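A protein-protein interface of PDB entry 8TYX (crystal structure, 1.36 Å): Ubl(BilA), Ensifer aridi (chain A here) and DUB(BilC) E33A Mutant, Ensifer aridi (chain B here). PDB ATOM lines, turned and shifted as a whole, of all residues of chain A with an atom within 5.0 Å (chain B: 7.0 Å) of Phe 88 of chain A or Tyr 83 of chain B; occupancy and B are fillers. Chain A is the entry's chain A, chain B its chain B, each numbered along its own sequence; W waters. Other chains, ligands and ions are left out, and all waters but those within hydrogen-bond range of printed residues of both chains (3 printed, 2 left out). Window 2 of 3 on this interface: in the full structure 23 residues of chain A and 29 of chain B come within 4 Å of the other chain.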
ATOM      1  N   ILE A  21       0.470 -32.232   2.359  1.00  0.00           N
ATOM      2  CA  ILE A  21       0.868 -30.845   2.164  1.00  0.00           C
ATOM      3  C   ILE A  21      -0.214 -29.994   2.809  1.00  0.00           C
ATOM      4  O   ILE A  21      -1.378 -30.047   2.396  1.00  0.00           O
ATOM      5  CB  ILE A  21       1.009 -30.484   0.680  1.00  0.00           C
ATOM      6  CG1 ILE A  21       2.059 -31.382   0.020  1.00  0.00           C
ATOM      7  CG2 ILE A  21       1.377 -29.007   0.505  1.00  0.00           C
ATOM      8  CD1 ILE A  21       2.131 -31.228  -1.497  1.00  0.00           C
ATOM      9  N   VAL A  23      -1.328 -26.108   3.567  1.00  0.00           N
ATOM     10  CA  VAL A  23      -1.117 -24.728   3.128  1.00  0.00           C
ATOM     11  C   VAL A  23      -1.715 -23.780   4.164  1.00  0.00           C
ATOM     12  O   VAL A  23      -2.901 -23.877   4.501  1.00  0.00           O
ATOM     13  CB  VAL A  23      -1.740 -24.523   1.726  1.00  0.00           C
ATOM     14  CG1 VAL A  23      -1.531 -23.069   1.286  1.00  0.00           C
ATOM     15  CG2 VAL A  23      -1.182 -25.518   0.720  1.00  0.00           C
ATOM     16  N   GLY A  26      -1.160 -19.401   2.265  1.00  0.00           N
ATOM     17  CA  GLY A  26      -0.536 -19.588   0.976  1.00  0.00           C
ATOM     18  C   GLY A  26       0.807 -20.289   0.983  1.00  0.00           C
ATOM     19  O   GLY A  26       1.386 -20.490  -0.096  1.00  0.00           O
ATOM     20  N   PRO A  28       3.067 -23.677   1.724  1.00  0.00           N
ATOM     21  CA  PRO A  28       2.941 -25.118   1.960  1.00  0.00           C
ATOM     22  C   PRO A  28       3.987 -25.639   2.934  1.00  0.00           C
ATOM     23  O   PRO A  28       5.120 -25.160   3.006  1.00  0.00           O
ATOM     24  CB  PRO A  28       3.179 -25.713   0.564  1.00  0.00           C
ATOM     25  CG  PRO A  28       4.153 -24.755  -0.067  1.00  0.00           C
ATOM     26  CD  PRO A  28       3.770 -23.381   0.462  1.00  0.00           C
ATOM     27  N   GLU A  61      -8.987 -24.215  11.131  1.00  0.00           N
ATOM     28  CA  GLU A  61      -9.741 -25.359  10.646  1.00  0.00           C
ATOM     29  C   GLU A  61      -9.270 -25.761   9.254  1.00  0.00           C
ATOM     30  O   GLU A  61      -8.749 -24.944   8.481  1.00  0.00           O
ATOM     31  CB  GLU A  61     -11.260 -25.085  10.683  1.00  0.00           C
ATOM     32  CG  GLU A  61     -11.700 -23.966   9.773  1.00  0.00           C
ATOM     33  CD  GLU A  61     -13.176 -23.672   9.853  1.00  0.00           C
ATOM     34  OE1 GLU A  61     -13.803 -23.944  10.903  1.00  0.00           O
ATOM     35  OE2 GLU A  61     -13.719 -23.193   8.837  1.00  0.00           O
ATOM     36  N   PHE A  62      -9.448 -27.043   8.960  1.00  0.00           N
ATOM     37  CA  PHE A  62      -9.008 -27.630   7.705  1.00  0.00           C
ATOM     38  C   PHE A  62     -10.136 -27.709   6.685  1.00  0.00           C
ATOM     39  O   PHE A  62     -11.255 -28.140   7.001  1.00  0.00           O
ATOM     40  CB  PHE A  62      -8.536 -29.075   7.916  1.00  0.00           C
ATOM     41  CG  PHE A  62      -7.146 -29.220   8.435  1.00  0.00           C
ATOM     42  CD1 PHE A  62      -6.053 -28.983   7.622  1.00  0.00           C
ATOM     43  CD2 PHE A  62      -6.927 -29.687   9.724  1.00  0.00           C
ATOM     44  CE1 PHE A  62      -4.759 -29.177   8.106  1.00  0.00           C
ATOM     45  CE2 PHE A  62      -5.647 -29.885  10.202  1.00  0.00           C
ATOM     46  CZ  PHE A  62      -4.571 -29.649   9.389  1.00  0.00           C
ATOM     47  N   LYS A  63      -9.799 -27.423   5.428  1.00  0.00           N
ATOM     48  CA  LYS A  63     -10.669 -27.699   4.290  1.00  0.00           C
ATOM     49  C   LYS A  63      -9.861 -28.416   3.228  1.00  0.00           C
ATOM     50  O   LYS A  63      -8.676 -28.147   3.056  1.00  0.00           O
ATOM     51  CB  LYS A  63     -11.239 -26.408   3.715  1.00  0.00           C
ATOM     52  CG  LYS A  63     -12.347 -25.825   4.565  1.00  0.00           C
ATOM     53  CD  LYS A  63     -13.299 -24.943   3.755  1.00  0.00           C
ATOM     54  CE  LYS A  63     -14.697 -25.001   4.357  1.00  0.00           C
ATOM     55  NZ  LYS A  63     -14.680 -24.669   5.812  1.00  0.00           N
ATOM     56  N   ASP A  64     -10.504 -29.345   2.528  1.00  0.00           N
ATOM     57  CA  ASP A  64      -9.832 -30.067   1.458  1.00  0.00           C
ATOM     58  C   ASP A  64      -9.835 -29.220   0.191  1.00  0.00           C
ATOM     59  O   ASP A  64     -10.270 -28.062   0.186  1.00  0.00           O
ATOM     60  CB  ASP A  64     -10.414 -31.476   1.273  1.00  0.00           C
ATOM     61  CG  ASP A  64     -11.877 -31.489   0.830  1.00  0.00           C
ATOM     62  OD1 ASP A  64     -12.380 -30.493   0.254  1.00  0.00           O
ATOM     63  OD2 ASP A  64     -12.525 -32.548   1.055  1.00  0.00           O
ATOM     64  N   GLU A  65      -9.313 -29.812  -0.894  1.00  0.00           N
ATOM     65  CA  GLU A  65      -9.238 -29.120  -2.176  1.00  0.00           C
ATOM     66  C   GLU A  65     -10.616 -28.909  -2.784  1.00  0.00           C
ATOM     67  O   GLU A  65     -10.832 -27.920  -3.493  1.00  0.00           O
ATOM     68  CB  GLU A  65      -8.336 -29.886  -3.152  1.00  0.00           C
ATOM     69  CG  GLU A  65      -6.837 -29.639  -2.938  1.00  0.00           C
ATOM     70  CD  GLU A  65      -5.982 -30.023  -4.134  1.00  0.00           C
ATOM     71  OE1 GLU A  65      -6.137 -31.145  -4.659  1.00  0.00           O
ATOM     72  OE2 GLU A  65      -5.142 -29.194  -4.552  1.00  0.00           O
ATOM     73  N   THR A  86      -3.326 -32.357  -0.591  1.00  0.00           N
ATOM     74  CA  THR A  86      -3.146 -30.986  -0.139  1.00  0.00           C
ATOM     75  C   THR A  86      -4.376 -30.542   0.642  1.00  0.00           C
ATOM     76  O   THR A  86      -5.509 -30.722   0.168  1.00  0.00           O
ATOM     77  CB  THR A  86      -2.918 -30.054  -1.334  1.00  0.00           C
ATOM     78  OG1 THR A  86      -1.721 -30.463  -2.020  1.00  0.00           O
ATOM     79  CG2 THR A  86      -2.768 -28.622  -0.883  1.00  0.00           C
ATOM     80  N   LEU A  87      -4.140 -30.006   1.844  1.00  0.00           N
ATOM     81  CA  LEU A  87      -5.188 -29.485   2.695  1.00  0.00           C
ATOM     82  C   LEU A  87      -4.898 -28.023   2.992  1.00  0.00           C
ATOM     83  O   LEU A  87      -3.733 -27.612   3.065  1.00  0.00           O
ATOM     84  CB  LEU A  87      -5.266 -30.219   4.018  1.00  0.00           C
ATOM     85  CG  LEU A  87      -5.570 -31.722   3.915  1.00  0.00           C
ATOM     86  CD1 LEU A  87      -5.615 -32.277   5.338  1.00  0.00           C
ATOM     87  CD2 LEU A  87      -6.844 -32.000   3.168  1.00  0.00           C
ATOM     88  N   PHE A  88      -5.958 -27.240   3.165  1.00  0.00           N
ATOM     89  CA  PHE A  88      -5.869 -25.822   3.480  1.00  0.00           C
ATOM     90  C   PHE A  88      -6.263 -25.594   4.934  1.00  0.00           C
ATOM     91  O   PHE A  88      -7.342 -26.010   5.373  1.00  0.00           O
ATOM     92  CB  PHE A  88      -6.720 -25.007   2.503  1.00  0.00           C
ATOM     93  CG  PHE A  88      -6.177 -25.055   1.102  1.00  0.00           C
ATOM     94  CD1 PHE A  88      -5.229 -24.147   0.680  1.00  0.00           C
ATOM     95  CD2 PHE A  88      -6.579 -26.041   0.233  1.00  0.00           C
ATOM     96  CE1 PHE A  88      -4.696 -24.214  -0.590  1.00  0.00           C
ATOM     97  CE2 PHE A  88      -6.056 -26.109  -1.053  1.00  0.00           C
ATOM     98  CZ  PHE A  88      -5.120 -25.206  -1.467  1.00  0.00           C
ATOM     99  N   LEU A  89      -5.375 -24.953   5.679  1.00  0.00           N
ATOM    100  CA  LEU A  89      -5.594 -24.705   7.083  1.00  0.00           C
ATOM    101  C   LEU A  89      -5.739 -23.196   7.240  1.00  0.00           C
ATOM    102  O   LEU A  89      -4.807 -22.433   6.921  1.00  0.00           O
ATOM    103  CB  LEU A  89      -4.404 -25.179   7.922  1.00  0.00           C
ATOM    104  CG  LEU A  89      -4.479 -25.033   9.446  1.00  0.00           C
ATOM    105  CD1 LEU A  89      -5.671 -25.830   9.979  1.00  0.00           C
ATOM    106  CD2 LEU A  89      -3.188 -25.492  10.110  1.00  0.00           C
ATOM    107  N   SER A  90      -6.911 -22.761   7.698  1.00  0.00           N
ATOM    108  CA  SER A  90      -7.242 -21.345   7.724  1.00  0.00           C
ATOM    109  C   SER A  90      -7.963 -20.967   9.007  1.00  0.00           C
ATOM    110  O   SER A  90      -8.537 -21.811   9.689  1.00  0.00           O
ATOM    111  CB  SER A  90      -8.136 -20.959   6.530  1.00  0.00           C
ATOM    112  OG  SER A  90      -7.712 -21.576   5.315  1.00  0.00           O
ATOM    113  N   HIS B  76     -10.488 -18.737   4.137  1.00  0.00           N
ATOM    114  CA  HIS B  76     -10.141 -19.862   3.288  1.00  0.00           C
ATOM    115  C   HIS B  76      -9.876 -19.401   1.862  1.00  0.00           C
ATOM    116  O   HIS B  76      -8.872 -19.798   1.256  1.00  0.00           O
ATOM    117  CB  HIS B  76     -11.257 -20.910   3.308  1.00  0.00           C
ATOM    118  CG  HIS B  76     -11.069 -22.000   2.302  1.00  0.00           C
ATOM    119  ND1 HIS B  76     -11.818 -22.096   1.147  1.00  0.00           N
ATOM    120  CD2 HIS B  76     -10.186 -23.022   2.269  1.00  0.00           C
ATOM    121  CE1 HIS B  76     -11.404 -23.138   0.450  1.00  0.00           C
ATOM    122  NE2 HIS B  76     -10.423 -23.718   1.113  1.00  0.00           N
ATOM    123  N   ARG B  77     -10.768 -18.576   1.304  1.00  0.00           N
ATOM    124  CA  ARG B  77     -10.550 -18.077  -0.053  1.00  0.00           C
ATOM    125  C   ARG B  77      -9.191 -17.396  -0.186  1.00  0.00           C
ATOM    126  O   ARG B  77      -8.470 -17.593  -1.177  1.00  0.00           O
ATOM    127  CB  ARG B  77     -11.661 -17.102  -0.448  1.00  0.00           C
ATOM    128  CG  ARG B  77     -11.589 -16.697  -1.910  1.00  0.00           C
ATOM    129  CD  ARG B  77     -12.280 -15.350  -2.206  1.00  0.00           C
ATOM    130  NE  ARG B  77     -11.661 -14.224  -1.514  1.00  0.00           N
ATOM    131  CZ  ARG B  77     -10.516 -13.648  -1.871  1.00  0.00           C
ATOM    132  NH1 ARG B  77      -9.840 -14.041  -2.945  1.00  0.00           N
ATOM    133  NH2 ARG B  77     -10.037 -12.642  -1.141  1.00  0.00           N
ATOM    134  N   LEU B  78      -8.837 -16.569   0.799  1.00  0.00           N
ATOM    135  CA  LEU B  78      -7.567 -15.851   0.781  1.00  0.00           C
ATOM    136  C   LEU B  78      -6.372 -16.803   0.808  1.00  0.00           C
ATOM    137  O   LEU B  78      -5.398 -16.611   0.084  1.00  0.00           O
ATOM    138  CB  LEU B  78      -7.503 -14.917   1.977  1.00  0.00           C
ATOM    139  CG  LEU B  78      -6.202 -14.151   2.174  1.00  0.00           C
ATOM    140  CD1 LEU B  78      -5.961 -13.173   1.037  1.00  0.00           C
ATOM    141  CD2 LEU B  78      -6.217 -13.456   3.570  1.00  0.00           C
ATOM    142  N   ASN B  79      -6.438 -17.843   1.630  1.00  0.00           N
ATOM    143  CA  ASN B  79      -5.381 -18.856   1.699  1.00  0.00           C
ATOM    144  C   ASN B  79      -5.160 -19.509   0.335  1.00  0.00           C
ATOM    145  O   ASN B  79      -4.028 -19.569  -0.171  1.00  0.00           O
ATOM    146  CB  ASN B  79      -5.783 -19.864   2.786  1.00  0.00           C
ATOM    147  CG  ASN B  79      -4.720 -20.892   3.103  1.00  0.00           C
ATOM    148  OD1 ASN B  79      -3.558 -20.797   2.691  1.00  0.00           O
ATOM    149  ND2 ASN B  79      -5.125 -21.893   3.864  1.00  0.00           N
ATOM    150  N   VAL B  80      -6.236 -19.990  -0.288  1.00  0.00           N
ATOM    151  CA  VAL B  80      -6.127 -20.649  -1.593  1.00  0.00           C
ATOM    152  C   VAL B  80      -5.587 -19.678  -2.630  1.00  0.00           C
ATOM    153  O   VAL B  80      -4.723 -20.032  -3.438  1.00  0.00           O
ATOM    154  CB  VAL B  80      -7.487 -21.239  -2.023  1.00  0.00           C
ATOM    155  CG1 VAL B  80      -7.414 -21.838  -3.439  1.00  0.00           C
ATOM    156  CG2 VAL B  80      -7.966 -22.296  -1.010  1.00  0.00           C
ATOM    157  N   TRP B  81      -6.063 -18.431  -2.588  1.00  0.00           N
ATOM    158  CA  TRP B  81      -5.645 -17.418  -3.555  1.00  0.00           C
ATOM    159  C   TRP B  81      -4.159 -17.097  -3.424  1.00  0.00           C
ATOM    160  O   TRP B  81      -3.432 -17.054  -4.426  1.00  0.00           O
ATOM    161  CB  TRP B  81      -6.507 -16.166  -3.327  1.00  0.00           C
ATOM    162  CG  TRP B  81      -6.210 -14.989  -4.196  1.00  0.00           C
ATOM    163  CD1 TRP B  81      -6.702 -14.763  -5.448  1.00  0.00           C
ATOM    164  CD2 TRP B  81      -5.399 -13.851  -3.881  1.00  0.00           C
ATOM    165  NE1 TRP B  81      -6.240 -13.563  -5.928  1.00  0.00           N
ATOM    166  CE2 TRP B  81      -5.423 -12.992  -4.994  1.00  0.00           C
ATOM    167  CE3 TRP B  81      -4.643 -13.475  -2.764  1.00  0.00           C
ATOM    168  CZ2 TRP B  81      -4.737 -11.787  -5.013  1.00  0.00           C
ATOM    169  CZ3 TRP B  81      -3.960 -12.285  -2.792  1.00  0.00           C
ATOM    170  CH2 TRP B  81      -4.020 -11.451  -3.902  1.00  0.00           C
ATOM    171  N   LEU B  82      -3.680 -16.890  -2.188  1.00  0.00           N
ATOM    172  CA  LEU B  82      -2.250 -16.673  -1.991  1.00  0.00           C
ATOM    173  C   LEU B  82      -1.432 -17.844  -2.537  1.00  0.00           C
ATOM    174  O   LEU B  82      -0.393 -17.643  -3.185  1.00  0.00           O
ATOM    175  CB  LEU B  82      -1.969 -16.492  -0.495  1.00  0.00           C
ATOM    176  CG  LEU B  82      -2.450 -15.215   0.184  1.00  0.00           C
ATOM    177  CD1 LEU B  82      -2.420 -15.405   1.682  1.00  0.00           C
ATOM    178  CD2 LEU B  82      -1.594 -14.040  -0.241  1.00  0.00           C
ATOM    179  N   TYR B  83      -1.886 -19.079  -2.287  1.00  0.00           N
ATOM    180  CA  TYR B  83      -1.170 -20.265  -2.756  1.00  0.00           C
ATOM    181  C   TYR B  83      -1.110 -20.299  -4.286  1.00  0.00           C
ATOM    182  O   TYR B  83      -0.051 -20.538  -4.880  1.00  0.00           O
ATOM    183  CB  TYR B  83      -1.886 -21.514  -2.244  1.00  0.00           C
ATOM    184  CG  TYR B  83      -1.193 -22.835  -2.493  1.00  0.00           C
ATOM    185  CD1 TYR B  83       0.145 -23.018  -2.152  1.00  0.00           C
ATOM    186  CD2 TYR B  83      -1.881 -23.913  -3.018  1.00  0.00           C
ATOM    187  CE1 TYR B  83       0.782 -24.230  -2.361  1.00  0.00           C
ATOM    188  CE2 TYR B  83      -1.248 -25.139  -3.228  1.00  0.00           C
ATOM    189  CZ  TYR B  83       0.079 -25.293  -2.861  1.00  0.00           C
ATOM    190  OH  TYR B  83       0.706 -26.508  -3.033  1.00  0.00           O
ATOM    191  N   LYS B  84      -2.242 -20.079  -4.959  1.00  0.00           N
ATOM    192  CA  LYS B  84      -2.238 -20.159  -6.421  1.00  0.00           C
ATOM    193  C   LYS B  84      -1.366 -19.060  -7.031  1.00  0.00           C
ATOM    194  O   LYS B  84      -0.740 -19.256  -8.083  1.00  0.00           O
ATOM    195  CB  LYS B  84      -3.668 -20.059  -6.969  1.00  0.00           C
ATOM    196  CG  LYS B  84      -4.607 -21.202  -6.609  1.00  0.00           C
ATOM    197  CD  LYS B  84      -4.119 -22.541  -7.054  1.00  0.00           C
ATOM    198  CE  LYS B  84      -5.154 -23.593  -6.711  1.00  0.00           C
ATOM    199  NZ  LYS B  84      -4.751 -24.903  -7.254  1.00  0.00           N
ATOM    200  N   ARG B  85      -1.347 -17.880  -6.414  1.00  0.00           N
ATOM    201  CA  ARG B  85      -0.640 -16.733  -6.963  1.00  0.00           C
ATOM    202  C   ARG B  85       0.821 -16.641  -6.534  1.00  0.00           C
ATOM    203  O   ARG B  85       1.543 -15.766  -7.038  1.00  0.00           O
ATOM    204  CB  ARG B  85      -1.357 -15.441  -6.529  1.00  0.00           C
ATOM    205  CG  ARG B  85      -2.798 -15.332  -7.047  1.00  0.00           C
ATOM    206  CD  ARG B  85      -2.878 -14.843  -8.482  1.00  0.00           C
ATOM    207  NE  ARG B  85      -2.407 -13.471  -8.621  1.00  0.00           N
ATOM    208  CZ  ARG B  85      -3.180 -12.393  -8.552  1.00  0.00           C
ATOM    209  NH1 ARG B  85      -4.487 -12.487  -8.353  1.00  0.00           N
ATOM    210  NH2 ARG B  85      -2.632 -11.190  -8.709  1.00  0.00           N
ATOM    211  N   GLY B  86       1.279 -17.502  -5.627  1.00  0.00           N
ATOM    212  CA  GLY B  86       2.634 -17.433  -5.124  1.00  0.00           C
ATOM    213  C   GLY B  86       2.911 -16.188  -4.301  1.00  0.00           C
ATOM    214  O   GLY B  86       4.025 -15.639  -4.361  1.00  0.00           O
ATOM    215  N   LEU B  87       1.934 -15.725  -3.522  1.00  0.00           N
ATOM    216  CA  LEU B  87       2.047 -14.502  -2.749  1.00  0.00           C
ATOM    217  C   LEU B  87       2.075 -14.826  -1.259  1.00  0.00           C
ATOM    218  O   LEU B  87       1.628 -15.883  -0.812  1.00  0.00           O
ATOM    219  CB  LEU B  87       0.891 -13.546  -3.068  1.00  0.00           C
ATOM    220  CG  LEU B  87       0.846 -12.991  -4.499  1.00  0.00           C
ATOM    221  CD1 LEU B  87      -0.462 -12.246  -4.758  1.00  0.00           C
ATOM    222  CD2 LEU B  87       2.052 -12.097  -4.754  1.00  0.00           C
HETATM  223  O   HOH W   1      -0.692 -28.729  -3.716  1.00  0.00           O
HETATM  224  O   HOH W   2      -4.448 -19.783   6.098  1.00  0.00           O
HETATM  225  O   HOH W   3      -6.973 -26.322  -5.036  1.00  0.00           O
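The backbone carbonyl oxygen (O) of Leu 87 of chain A lies within hydrogen-bond range of the backbone NH (N) of Val 23 of chain A.
The backbone carbonyl oxygen (O) of Val 23 of chain A lies within hydrogen-bond range of the backbone NH (N) of Leu 89 of chain A.
The side-chain carboxylate (OE2) of Glu 61 of chain A lies within salt-bridge range of the side-chain amino group (NZ) of Lys 63 of chain A (3.5 Å).
N of Glu 61 of chain A sits at hydrogen-bond distance from O of Ser 90 of chain A (2.8 Å).
The backbone NH of Lys 63 of chain A sits at hydrogen-bond distance from the backbone carbonyl oxygen of Phe 88 of chain A, at 2.8 Å.
The backbone carbonyl oxygen (O) of Leu 82 of chain B sits at hydrogen-bond distance from the backbone NH (N) of Leu 87 of chain B.
Among the printed residues, merely in contact across the chains: Gly 26 of chain A with Tyr 83 of chain B (3.5 Å), Ser 90 of chain A with His 76 of chain B (3.6 Å), Phe 88 of chain A with Val 80 of chain B (3.7 Å), Gly 26 of chain A with Leu 82 of chain B (3.7 Å), Phe 88 of chain A with Tyr 83 of chain B (3.7 Å), Phe 88 of chain A with Asn 79 of chain B (3.8 Å), Val 23 of chain A with Tyr 83 of chain B (3.8 Å) and Lys 63 of chain A with His 76 of chain B (3.8 Å).
Tyr 83 of chain B touches just these residues of chain A: Val 23, Gly 26 and Phe 88.
Printed residues of chain B within 4 Å of Leu 89 of chain A: Asn 79.
Printed residues of chain B within 4 Å of Gly 26 of chain A: Asn 79, Leu 82 and Tyr 83.
Printed residues of chain A within 4 Å of Asn 79 of chain B: Val 23 (3.0 Å), Gly 26 (2.8 Å), Phe 88 (3.8 Å), Leu 89 (3.1 Å) and Ser 90 (3.0 Å).
Printed residues of chain A within 4 Å of His 76 of chain B: Lys 63 and Ser 90.
Thr 86 of chain A touches none of the printed residues of chain B.
The nearest printed residue of chain B that does not touch Phe 88 of chain A is His 76 of chain B (4.001 Å).
The nearest residue of chain A that does not touch Tyr 83 of chain B is Pro 28 of chain A (4.1 Å).
The side-chain amide nitrogen (ND2) of Asn 79 of chain B is in hydrogen-bond range of the backbone carbonyl oxygen (O) of Val 23 of chain A, 3.0 Å away.
The backbone NH of Gly 26 of chain A lies within hydrogen-bond range of the side-chain amide oxygen of Asn 79 of chain B, at 2.8 Å.
ND2 of Asn 79 of chain B is in hydrogen-bond range of O of Leu 89 of chain A (3.1 Å).
The side-chain hydroxyl (OG) of Ser 90 of chain A lies within hydrogen-bond range of the side-chain amide nitrogen (ND2) of Asn 79 of chain B.
Of the 12 printed residues of chain B, 5 touch a printed residue of chain A.
Hydrophobic or aromatic side chains of chain B that line the printed part of chain A: His 76, Val 80, Leu 82 and Tyr 83.
Of the 14 printed residues of chain A, 6 touch a printed residue of chain B.
Among the printed residues, 12 pairs touch across the chains.
Water W1 lies within hydrogen-bond range of OG1 of Thr 86 of chain A and OH of Tyr 83 of chain B.
Water W2 bridges the backbone carbonyl oxygen of Leu 89 of chain A (2.8 Å) and the side-chain amide nitrogen of Asn 79 of chain B (3.1 Å).
Water W3 bridges OE2 of Glu 65 of chain A (3.4 Å) and NZ of Lys 84 of chain B (3.4 Å).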
